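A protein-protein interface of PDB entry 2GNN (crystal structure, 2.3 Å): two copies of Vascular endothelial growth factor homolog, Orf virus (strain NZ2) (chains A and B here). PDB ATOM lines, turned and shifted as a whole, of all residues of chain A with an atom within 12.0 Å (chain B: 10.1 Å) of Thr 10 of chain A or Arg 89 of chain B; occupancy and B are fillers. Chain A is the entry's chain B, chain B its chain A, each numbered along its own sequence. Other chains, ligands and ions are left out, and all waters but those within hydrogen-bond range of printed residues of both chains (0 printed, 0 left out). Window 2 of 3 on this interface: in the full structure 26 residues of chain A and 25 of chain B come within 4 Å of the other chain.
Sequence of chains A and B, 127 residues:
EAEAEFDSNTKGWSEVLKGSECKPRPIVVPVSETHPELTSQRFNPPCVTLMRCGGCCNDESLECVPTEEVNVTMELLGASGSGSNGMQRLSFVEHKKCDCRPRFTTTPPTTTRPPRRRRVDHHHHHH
The backbone carbonyl oxygen of Asn 44 of chain B is in hydrogen-bond range of the indole nitrogen of Trp 13 of chain A, at 3.1 Å. The backbone carbonyl oxygen of Thr 73 of chain B sits at hydrogen-bond distance from the backbone NH of Lys 11 of chain A, at 2.8 Å. O of Lys 11 of chain A lies within hydrogen-bond range of N of Glu 75 of chain B (3.0 Å). The side-chain carboxylate (OE1) of Glu 75 of chain B sits at hydrogen-bond distance from the backbone NH (N) of Trp 13 of chain A (3.3 Å). The guanidinium group of Arg 89 of chain B is in hydrogen-bond range of the side-chain hydroxyl of Thr 10 of chain A (2.6 Å).
O of Asn 44 of chain B is in hydrogen-bond range of N of Leu 77 of chain B, at 2.9 Å. The backbone carbonyl oxygen (O) of Val 72 of chain B sits at hydrogen-bond distance from the backbone NH (N) of Phe 92 of chain B. O of Leu 90 of chain B is in hydrogen-bond range of N of Met 74 of chain B (2.9 Å). The side-chain sulfur (SD) of Met 87 of chain B lies close to the backbone NH (N) of Leu 76 of chain B, 3.8 Å away.
Among the printed residues, pairs that only touch across the chains: Val 16 of chain A with Glu 75 of chain B (3.4 Å), Thr 10 of chain A with Thr 73 of chain B (3.5 Å), Lys 11 of chain A with Met 74 of chain B (3.5 Å), Gly 12 of chain A with Glu 75 of chain B (3.5 Å), Val 16 of chain A with Met 74 of chain B (3.7 Å), Trp 13 of chain A with Met 87 of chain B (3.8 Å), Lys 11 of chain A with Val 72 of chain B (3.9 Å), Val 16 of chain A with Val 48 of chain B (3.99 Å) and Leu 17 of chain A with Asn 44 of chain B (3.99 Å).
Arg 89 of chain B touches just one residue of chain A: Thr 10 (2.6 Å). No residue of chain B comes within 4 Å of Asn 9 of chain A. Of chain A, only Thr 10 and Lys 11 come within 4 Å of Thr 73 of chain B. Of chain A, only Lys 11, Gly 12, Trp 13 and Val 16 come within 4 Å of Glu 75 of chain B. No residue of chain A comes within 4 Å of Leu 76 of chain B. No residue of chain A comes within 4 Å of Gln 88 of chain B. No residue of chain A comes within 4 Å of Leu 90 of chain B. No residue of chain A comes within 4 Å of Ser 91 of chain B. Of the printed residues of chain B, Val 16 of chain A touches Val 48 (3.99 Å), Met 74 (3.7 Å) and Glu 75 (3.4 Å). Of the printed residues of chain A, Val 48 of chain B touches Val 16 (3.99 Å). Of the printed residues of chain A, Met 87 of chain B touches Trp 13. Of the printed residues of chain A, Met 74 of chain B touches Lys 11 (3.5 Å) and Val 16 (3.7 Å). Ser 14 of chain A touches none of the printed residues of chain B. His 35 of chain B touches none of the printed residues of chain A. The nearest residue of chain A that does not touch Arg 89 of chain B is Asn 9 of chain A (5.7 Å). The nearest printed residue of chain B that does not touch Trp 13 of chain A is Leu 77 of chain B (4.1 Å).
Of the 23 printed residues of chain B, 8 touch a printed residue of chain A. Of the 9 printed residues of chain A, 6 touch a printed residue of chain B. Along chain A the printed residues that touch a printed residue of chain B span positions 10 to 17.
No position is printed for both chains. Of the 14 pairs that touch across the chains among the printed residues, none has its exchanged pair printed and touching as well.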
ATOM      1  N   ASN A   9       1.055   8.178   5.387  1.00  0.00           N
ATOM      2  CA  ASN A   9       1.849   7.519   4.305  1.00  0.00           C
ATOM      3  C   ASN A   9       3.284   8.080   4.148  1.00  0.00           C
ATOM      4  O   ASN A   9       3.731   8.937   4.935  1.00  0.00           O
ATOM      5  CB  ASN A   9       1.083   7.575   2.975  1.00  0.00           C
ATOM      6  CG  ASN A   9       1.285   6.327   2.126  1.00  0.00           C
ATOM      7  OD1 ASN A   9       1.227   5.203   2.629  1.00  0.00           O
ATOM      8  ND2 ASN A   9       1.511   6.521   0.829  1.00  0.00           N
ATOM      9  N   THR A  10       3.987   7.570   3.133  1.00  0.00           N
ATOM     10  CA  THR A  10       5.395   7.881   2.850  1.00  0.00           C
ATOM     11  C   THR A  10       5.589   9.300   2.310  1.00  0.00           C
ATOM     12  O   THR A  10       4.844   9.737   1.435  1.00  0.00           O
ATOM     13  CB  THR A  10       5.968   6.879   1.800  1.00  0.00           C
ATOM     14  OG1 THR A  10       5.635   5.537   2.172  1.00  0.00           O
ATOM     15  CG2 THR A  10       7.485   7.005   1.657  1.00  0.00           C
ATOM     16  N   LYS A  11       6.596  10.005   2.826  1.00  0.00           N
ATOM     17  CA  LYS A  11       7.029  11.282   2.238  1.00  0.00           C
ATOM     18  C   LYS A  11       7.960  11.067   1.031  1.00  0.00           C
ATOM     19  O   LYS A  11       9.019  10.444   1.150  1.00  0.00           O
ATOM     20  CB  LYS A  11       7.690  12.171   3.287  1.00  0.00           C
ATOM     21  CG  LYS A  11       6.727  12.692   4.341  1.00  0.00           C
ATOM     22  CD  LYS A  11       7.399  13.701   5.257  1.00  0.00           C
ATOM     23  CE  LYS A  11       6.452  14.145   6.371  1.00  0.00           C
ATOM     24  NZ  LYS A  11       7.090  15.115   7.310  1.00  0.00           N
ATOM     25  N   GLY A  12       7.541  11.567  -0.132  1.00  0.00           N
ATOM     26  CA  GLY A  12       8.327  11.458  -1.359  1.00  0.00           C
ATOM     27  C   GLY A  12       9.609  12.280  -1.337  1.00  0.00           C
ATOM     28  O   GLY A  12       9.713  13.286  -0.622  1.00  0.00           O
ATOM     29  N   TRP A  13      10.583  11.848  -2.134  1.00  0.00           N
ATOM     30  CA  TRP A  13      11.927  12.434  -2.133  1.00  0.00           C
ATOM     31  C   TRP A  13      11.996  13.963  -2.288  1.00  0.00           C
ATOM     32  O   TRP A  13      12.765  14.615  -1.576  1.00  0.00           O
ATOM     33  CB  TRP A  13      12.821  11.747  -3.170  1.00  0.00           C
ATOM     34  CG  TRP A  13      14.206  12.292  -3.174  1.00  0.00           C
ATOM     35  CD1 TRP A  13      15.176  12.065  -2.241  1.00  0.00           C
ATOM     36  CD2 TRP A  13      14.777  13.179  -4.145  1.00  0.00           C
ATOM     37  NE1 TRP A  13      16.322  12.749  -2.575  1.00  0.00           N
ATOM     38  CE2 TRP A  13      16.105  13.442  -3.739  1.00  0.00           C
ATOM     39  CE3 TRP A  13      14.298  13.770  -5.328  1.00  0.00           C
ATOM     40  CZ2 TRP A  13      16.960  14.278  -4.465  1.00  0.00           C
ATOM     41  CZ3 TRP A  13      15.150  14.598  -6.054  1.00  0.00           C
ATOM     42  CH2 TRP A  13      16.467  14.843  -5.618  1.00  0.00           C
ATOM     43  N   SER A  14      11.208  14.526  -3.207  1.00  0.00           N
ATOM     44  CA  SER A  14      11.150  15.982  -3.385  1.00  0.00           C
ATOM     45  C   SER A  14      10.792  16.676  -2.077  1.00  0.00           C
ATOM     46  O   SER A  14      11.458  17.636  -1.672  1.00  0.00           O
ATOM     47  CB  SER A  14      10.158  16.385  -4.477  1.00  0.00           C
ATOM     48  OG  SER A  14      10.634  16.034  -5.770  1.00  0.00           O
ATOM     49  N   GLU A  15       9.756  16.175  -1.406  1.00  0.00           N
ATOM     50  CA  GLU A  15       9.336  16.730  -0.123  1.00  0.00           C
ATOM     51  C   GLU A  15      10.434  16.578   0.934  1.00  0.00           C
ATOM     52  O   GLU A  15      10.638  17.479   1.753  1.00  0.00           O
ATOM     53  CB  GLU A  15       8.029  16.081   0.349  1.00  0.00           C
ATOM     54  CG  GLU A  15       7.202  16.978   1.279  1.00  0.00           C
ATOM     55  CD  GLU A  15       6.295  16.199   2.229  1.00  0.00           C
ATOM     56  OE1 GLU A  15       5.485  15.374   1.756  1.00  0.00           O
ATOM     57  OE2 GLU A  15       6.390  16.428   3.456  1.00  0.00           O
ATOM     58  N   VAL A  16      11.142  15.447   0.902  1.00  0.00           N
ATOM     59  CA  VAL A  16      12.214  15.167   1.868  1.00  0.00           C
ATOM     60  C   VAL A  16      13.380  16.139   1.676  1.00  0.00           C
ATOM     61  O   VAL A  16      13.900  16.708   2.642  1.00  0.00           O
ATOM     62  CB  VAL A  16      12.714  13.692   1.783  1.00  0.00           C
ATOM     63  CG1 VAL A  16      13.880  13.459   2.736  1.00  0.00           C
ATOM     64  CG2 VAL A  16      11.591  12.724   2.105  1.00  0.00           C
ATOM     65  N   LEU A  17      13.768  16.325   0.416  1.00  0.00           N
ATOM     66  CA  LEU A  17      14.822  17.253   0.034  1.00  0.00           C
ATOM     67  C   LEU A  17      14.471  18.675   0.456  1.00  0.00           C
ATOM     68  O   LEU A  17      15.250  19.334   1.141  1.00  0.00           O
ATOM     69  CB  LEU A  17      15.053  17.174  -1.472  1.00  0.00           C
ATOM     70  CG  LEU A  17      16.193  18.005  -2.051  1.00  0.00           C
ATOM     71  CD1 LEU A  17      17.540  17.338  -1.777  1.00  0.00           C
ATOM     72  CD2 LEU A  17      15.968  18.207  -3.537  1.00  0.00           C
ATOM     73  N   VAL B  31      20.948  11.953   9.129  1.00  0.00           N
ATOM     74  CA  VAL B  31      20.536  10.563   8.931  1.00  0.00           C
ATOM     75  C   VAL B  31      21.484   9.578   9.626  1.00  0.00           C
ATOM     76  O   VAL B  31      21.034   8.595  10.219  1.00  0.00           O
ATOM     77  CB  VAL B  31      20.391  10.208   7.427  1.00  0.00           C
ATOM     78  CG1 VAL B  31      19.926   8.778   7.260  1.00  0.00           C
ATOM     79  CG2 VAL B  31      19.413  11.146   6.747  1.00  0.00           C
ATOM     80  N   HIS B  35      19.987   6.321  12.066  1.00  0.00           N
ATOM     81  CA  HIS B  35      20.146   4.922  11.702  1.00  0.00           C
ATOM     82  C   HIS B  35      21.625   4.538  11.827  1.00  0.00           C
ATOM     83  O   HIS B  35      22.358   4.563  10.833  1.00  0.00           O
ATOM     84  CB  HIS B  35      19.643   4.673  10.271  1.00  0.00           C
ATOM     85  CG  HIS B  35      18.158   4.806  10.108  1.00  0.00           C
ATOM     86  ND1 HIS B  35      17.481   5.984  10.343  1.00  0.00           N
ATOM     87  CD2 HIS B  35      17.222   3.911   9.706  1.00  0.00           C
ATOM     88  CE1 HIS B  35      16.194   5.807  10.105  1.00  0.00           C
ATOM     89  NE2 HIS B  35      16.009   4.558   9.718  1.00  0.00           N
ATOM     90  N   GLU B  37      22.961   1.814  12.019  1.00  0.00           N
ATOM     91  CA  GLU B  37      23.229   0.513  11.398  1.00  0.00           C
ATOM     92  C   GLU B  37      23.602   0.647   9.920  1.00  0.00           C
ATOM     93  O   GLU B  37      23.977  -0.338   9.273  1.00  0.00           O
ATOM     94  CB  GLU B  37      22.026  -0.430  11.563  1.00  0.00           C
ATOM     95  CG  GLU B  37      20.856  -0.186  10.596  1.00  0.00           C
ATOM     96  CD  GLU B  37      19.988   1.011  10.968  1.00  0.00           C
ATOM     97  OE1 GLU B  37      20.224   1.636  12.024  1.00  0.00           O
ATOM     98  OE2 GLU B  37      19.055   1.322  10.198  1.00  0.00           O
ATOM     99  N   LEU B  38      23.492   1.866   9.396  1.00  0.00           N
ATOM    100  CA  LEU B  38      23.785   2.134   7.987  1.00  0.00           C
ATOM    101  C   LEU B  38      24.746   3.314   7.760  1.00  0.00           C
ATOM    102  O   LEU B  38      24.769   3.901   6.672  1.00  0.00           O
ATOM    103  CB  LEU B  38      22.483   2.319   7.190  1.00  0.00           C
ATOM    104  CG  LEU B  38      21.723   1.061   6.747  1.00  0.00           C
ATOM    105  CD1 LEU B  38      20.331   1.439   6.259  1.00  0.00           C
ATOM    106  CD2 LEU B  38      22.488   0.270   5.675  1.00  0.00           C
ATOM    107  N   GLN B  41      27.101   4.200   4.778  1.00  0.00           N
ATOM    108  CA  GLN B  41      26.488   4.776   3.579  1.00  0.00           C
ATOM    109  C   GLN B  41      26.172   6.267   3.751  1.00  0.00           C
ATOM    110  O   GLN B  41      25.817   6.714   4.847  1.00  0.00           O
ATOM    111  CB  GLN B  41      25.212   4.001   3.229  1.00  0.00           C
ATOM    112  CG  GLN B  41      24.735   4.170   1.789  1.00  0.00           C
ATOM    113  CD  GLN B  41      23.604   3.223   1.427  1.00  0.00           C
ATOM    114  OE1 GLN B  41      22.946   2.648   2.300  1.00  0.00           O
ATOM    115  NE2 GLN B  41      23.371   3.054   0.130  1.00  0.00           N
ATOM    116  N   PHE B  43      23.739   9.499   2.398  1.00  0.00           N
ATOM    117  CA  PHE B  43      22.385   9.692   1.876  1.00  0.00           C
ATOM    118  C   PHE B  43      22.147  11.078   1.301  1.00  0.00           C
ATOM    119  O   PHE B  43      22.614  12.076   1.845  1.00  0.00           O
ATOM    120  CB  PHE B  43      21.339   9.411   2.959  1.00  0.00           C
ATOM    121  CG  PHE B  43      21.129   7.958   3.223  1.00  0.00           C
ATOM    122  CD1 PHE B  43      20.465   7.158   2.294  1.00  0.00           C
ATOM    123  CD2 PHE B  43      21.602   7.378   4.393  1.00  0.00           C
ATOM    124  CE1 PHE B  43      20.274   5.800   2.527  1.00  0.00           C
ATOM    125  CE2 PHE B  43      21.413   6.023   4.641  1.00  0.00           C
ATOM    126  CZ  PHE B  43      20.750   5.230   3.704  1.00  0.00           C
ATOM    127  N   ASN B  44      21.409  11.117   0.196  1.00  0.00           N
ATOM    128  CA  ASN B  44      20.960  12.363  -0.397  1.00  0.00           C
ATOM    129  C   ASN B  44      19.448  12.497  -0.211  1.00  0.00           C
ATOM    130  O   ASN B  44      18.682  11.760  -0.838  1.00  0.00           O
ATOM    131  CB  ASN B  44      21.335  12.406  -1.885  1.00  0.00           C
ATOM    132  CG  ASN B  44      21.223  13.798  -2.489  1.00  0.00           C
ATOM    133  OD1 ASN B  44      20.476  14.647  -2.006  1.00  0.00           O
ATOM    134  ND2 ASN B  44      21.969  14.032  -3.561  1.00  0.00           N
ATOM    135  N   VAL B  48      17.207  15.148   7.619  1.00  0.00           N
ATOM    136  CA  VAL B  48      15.764  15.299   7.456  1.00  0.00           C
ATOM    137  C   VAL B  48      15.201  16.200   8.533  1.00  0.00           C
ATOM    138  O   VAL B  48      15.804  16.350   9.595  1.00  0.00           O
ATOM    139  CB  VAL B  48      15.028  13.925   7.515  1.00  0.00           C
ATOM    140  CG1 VAL B  48      15.467  13.034   6.371  1.00  0.00           C
ATOM    141  CG2 VAL B  48      15.256  13.224   8.854  1.00  0.00           C
ATOM    142  N   ASN B  71       5.244   6.845  13.582  1.00  0.00           N
ATOM    143  CA  ASN B  71       6.249   6.618  12.554  1.00  0.00           C
ATOM    144  C   ASN B  71       5.994   7.432  11.306  1.00  0.00           C
ATOM    145  O   ASN B  71       4.844   7.627  10.908  1.00  0.00           O
ATOM    146  CB  ASN B  71       6.314   5.146  12.154  1.00  0.00           C
ATOM    147  CG  ASN B  71       6.796   4.260  13.273  1.00  0.00           C
ATOM    148  OD1 ASN B  71       7.525   4.712  14.162  1.00  0.00           O
ATOM    149  ND2 ASN B  71       6.388   2.989  13.246  1.00  0.00           N
ATOM    150  N   VAL B  72       7.077   7.893  10.683  1.00  0.00           N
ATOM    151  CA  VAL B  72       7.016   8.518   9.370  1.00  0.00           C
ATOM    152  C   VAL B  72       8.024   7.813   8.478  1.00  0.00           C
ATOM    153  O   VAL B  72       9.153   7.548   8.889  1.00  0.00           O
ATOM    154  CB  VAL B  72       7.295  10.038   9.441  1.00  0.00           C
ATOM    155  CG1 VAL B  72       7.136  10.679   8.085  1.00  0.00           C
ATOM    156  CG2 VAL B  72       6.318  10.695  10.379  1.00  0.00           C
ATOM    157  N   THR B  73       7.605   7.475   7.266  1.00  0.00           N
ATOM    158  CA  THR B  73       8.525   6.896   6.308  1.00  0.00           C
ATOM    159  C   THR B  73       8.899   7.974   5.302  1.00  0.00           C
ATOM    160  O   THR B  73       8.072   8.819   4.945  1.00  0.00           O
ATOM    161  CB  THR B  73       7.925   5.663   5.605  1.00  0.00           C
ATOM    162  OG1 THR B  73       7.520   4.704   6.585  1.00  0.00           O
ATOM    163  CG2 THR B  73       8.943   5.011   4.702  1.00  0.00           C
ATOM    164  N   MET B  74      10.154   7.951   4.863  1.00  0.00           N
ATOM    165  CA  MET B  74      10.667   8.917   3.889  1.00  0.00           C
ATOM    166  C   MET B  74      11.544   8.222   2.869  1.00  0.00           C
ATOM    167  O   MET B  74      12.317   7.332   3.223  1.00  0.00           O
ATOM    168  CB  MET B  74      11.480  10.010   4.591  1.00  0.00           C
ATOM    169  CG  MET B  74      10.745  10.706   5.719  1.00  0.00           C
ATOM    170  SD  MET B  74      11.663  12.106   6.326  1.00  0.00           S
ATOM    171  CE  MET B  74      10.739  12.582   7.771  1.00  0.00           C
ATOM    172  N   GLU B  75      11.411   8.629   1.608  1.00  0.00           N
ATOM    173  CA  GLU B  75      12.313   8.212   0.543  1.00  0.00           C
ATOM    174  C   GLU B  75      13.610   9.030   0.596  1.00  0.00           C
ATOM    175  O   GLU B  75      13.580  10.252   0.768  1.00  0.00           O
ATOM    176  CB  GLU B  75      11.643   8.401  -0.817  1.00  0.00           C
ATOM    177  CG  GLU B  75      10.490   7.446  -1.122  1.00  0.00           C
ATOM    178  CD  GLU B  75       9.946   7.625  -2.538  1.00  0.00           C
ATOM    179  OE1 GLU B  75       9.932   8.775  -3.039  1.00  0.00           O
ATOM    180  OE2 GLU B  75       9.537   6.614  -3.156  1.00  0.00           O
ATOM    181  N   LEU B  76      14.745   8.347   0.464  1.00  0.00           N
ATOM    182  CA  LEU B  76      16.062   8.985   0.417  1.00  0.00           C
ATOM    183  C   LEU B  76      16.952   8.283  -0.594  1.00  0.00           C
ATOM    184  O   LEU B  76      16.863   7.073  -0.757  1.00  0.00           O
ATOM    185  CB  LEU B  76      16.743   8.943   1.785  1.00  0.00           C
ATOM    186  CG  LEU B  76      16.300   9.936   2.859  1.00  0.00           C
ATOM    187  CD1 LEU B  76      15.223   9.341   3.733  1.00  0.00           C
ATOM    188  CD2 LEU B  76      17.482  10.325   3.712  1.00  0.00           C
ATOM    189  N   LEU B  77      17.814   9.041  -1.266  1.00  0.00           N
ATOM    190  CA  LEU B  77      18.760   8.460  -2.214  1.00  0.00           C
ATOM    191  C   LEU B  77      19.963   7.825  -1.523  1.00  0.00           C
ATOM    192  O   LEU B  77      20.608   8.451  -0.686  1.00  0.00           O
ATOM    193  CB  LEU B  77      19.233   9.503  -3.232  1.00  0.00           C
ATOM    194  CG  LEU B  77      18.571   9.574  -4.612  1.00  0.00           C
ATOM    195  CD1 LEU B  77      19.345  10.532  -5.493  1.00  0.00           C
ATOM    196  CD2 LEU B  77      18.503   8.211  -5.286  1.00  0.00           C
ATOM    197  N   GLY B  78      20.260   6.581  -1.894  1.00  0.00           N
ATOM    198  CA  GLY B  78      21.415   5.853  -1.363  1.00  0.00           C
ATOM    199  C   GLY B  78      22.720   6.231  -2.035  1.00  0.00           C
ATOM    200  O   GLY B  78      23.245   5.486  -2.865  1.00  0.00           O
ATOM    201  N   GLY B  86      19.648   2.283  -5.176  1.00  0.00           N
ATOM    202  CA  GLY B  86      18.849   3.458  -5.503  1.00  0.00           C
ATOM    203  C   GLY B  86      18.113   4.052  -4.312  1.00  0.00           C
ATOM    204  O   GLY B  86      18.690   4.240  -3.234  1.00  0.00           O
ATOM    205  N   MET B  87      16.831   4.348  -4.519  1.00  0.00           N
ATOM    206  CA  MET B  87      15.982   4.991  -3.513  1.00  0.00           C
ATOM    207  C   MET B  87      15.617   4.035  -2.370  1.00  0.00           C
ATOM    208  O   MET B  87      15.246   2.884  -2.599  1.00  0.00           O
ATOM    209  CB  MET B  87      14.712   5.532  -4.176  1.00  0.00           C
ATOM    210  CG  MET B  87      13.913   6.510  -3.331  1.00  0.00           C
ATOM    211  SD  MET B  87      14.600   8.179  -3.323  1.00  0.00           S
ATOM    212  CE  MET B  87      14.170   8.710  -4.983  1.00  0.00           C
ATOM    213  N   GLN B  88      15.716   4.529  -1.140  1.00  0.00           N
ATOM    214  CA  GLN B  88      15.461   3.724   0.045  1.00  0.00           C
ATOM    215  C   GLN B  88      14.441   4.397   0.940  1.00  0.00           C
ATOM    216  O   GLN B  88      14.448   5.622   1.087  1.00  0.00           O
ATOM    217  CB  GLN B  88      16.757   3.506   0.830  1.00  0.00           C
ATOM    218  CG  GLN B  88      17.767   2.594   0.135  1.00  0.00           C
ATOM    219  CD  GLN B  88      19.053   2.404   0.930  1.00  0.00           C
ATOM    220  OE1 GLN B  88      20.083   2.020   0.371  1.00  0.00           O
ATOM    221  NE2 GLN B  88      18.999   2.666   2.238  1.00  0.00           N
ATOM    222  N   ARG B  89      13.569   3.587   1.539  1.00  0.00           N
ATOM    223  CA  ARG B  89      12.629   4.071   2.543  1.00  0.00           C
ATOM    224  C   ARG B  89      13.235   3.905   3.923  1.00  0.00           C
ATOM    225  O   ARG B  89      13.634   2.805   4.316  1.00  0.00           O
ATOM    226  CB  ARG B  89      11.298   3.322   2.470  1.00  0.00           C
ATOM    227  CG  ARG B  89      10.584   3.438   1.145  1.00  0.00           C
ATOM    228  CD  ARG B  89       9.089   3.311   1.321  1.00  0.00           C
ATOM    229  NE  ARG B  89       8.407   3.319   0.030  1.00  0.00           N
ATOM    230  CZ  ARG B  89       7.085   3.326  -0.126  1.00  0.00           C
ATOM    231  NH1 ARG B  89       6.281   3.327   0.935  1.00  0.00           N
ATOM    232  NH2 ARG B  89       6.567   3.329  -1.348  1.00  0.00           N
ATOM    233  N   LEU B  90      13.328   5.010   4.648  1.00  0.00           N
ATOM    234  CA  LEU B  90      13.759   4.964   6.025  1.00  0.00           C
ATOM    235  C   LEU B  90      12.617   5.449   6.906  1.00  0.00           C
ATOM    236  O   LEU B  90      11.857   6.353   6.529  1.00  0.00           O
ATOM    237  CB  LEU B  90      15.027   5.794   6.256  1.00  0.00           C
ATOM    238  CG  LEU B  90      16.290   5.532   5.414  1.00  0.00           C
ATOM    239  CD1 LEU B  90      17.391   6.495   5.837  1.00  0.00           C
ATOM    240  CD2 LEU B  90      16.791   4.087   5.491  1.00  0.00           C
ATOM    241  N   SER B  91      12.497   4.826   8.074  1.00  0.00           N
ATOM    242  CA  SER B  91      11.440   5.141   9.012  1.00  0.00           C
ATOM    243  C   SER B  91      12.034   5.931  10.169  1.00  0.00           C
ATOM    244  O   SER B  91      13.166   5.688  10.584  1.00  0.00           O
ATOM    245  CB  SER B  91      10.772   3.842   9.485  1.00  0.00           C
ATOM    246  OG  SER B  91       9.710   4.093  10.396  1.00  0.00           O
ATOM    247  N   PHE B  92      11.268   6.890  10.673  1.00  0.00           N
ATOM    248  CA  PHE B  92      11.703   7.783  11.725  1.00  0.00           C
ATOM    249  C   PHE B  92      10.547   7.917  12.714  1.00  0.00           C
ATOM    250  O   PHE B  92       9.401   7.673  12.348  1.00  0.00           O
ATOM    251  CB  PHE B  92      12.009   9.167  11.143  1.00  0.00           C
ATOM    252  CG  PHE B  92      13.142   9.189  10.149  1.00  0.00           C
ATOM    253  CD1 PHE B  92      14.455   9.353  10.576  1.00  0.00           C
ATOM    254  CD2 PHE B  92      12.894   9.062   8.778  1.00  0.00           C
ATOM    255  CE1 PHE B  92      15.511   9.379   9.657  1.00  0.00           C
ATOM    256  CE2 PHE B  92      13.936   9.091   7.853  1.00  0.00           C
ATOM    257  CZ  PHE B  92      15.246   9.245   8.289  1.00  0.00           C
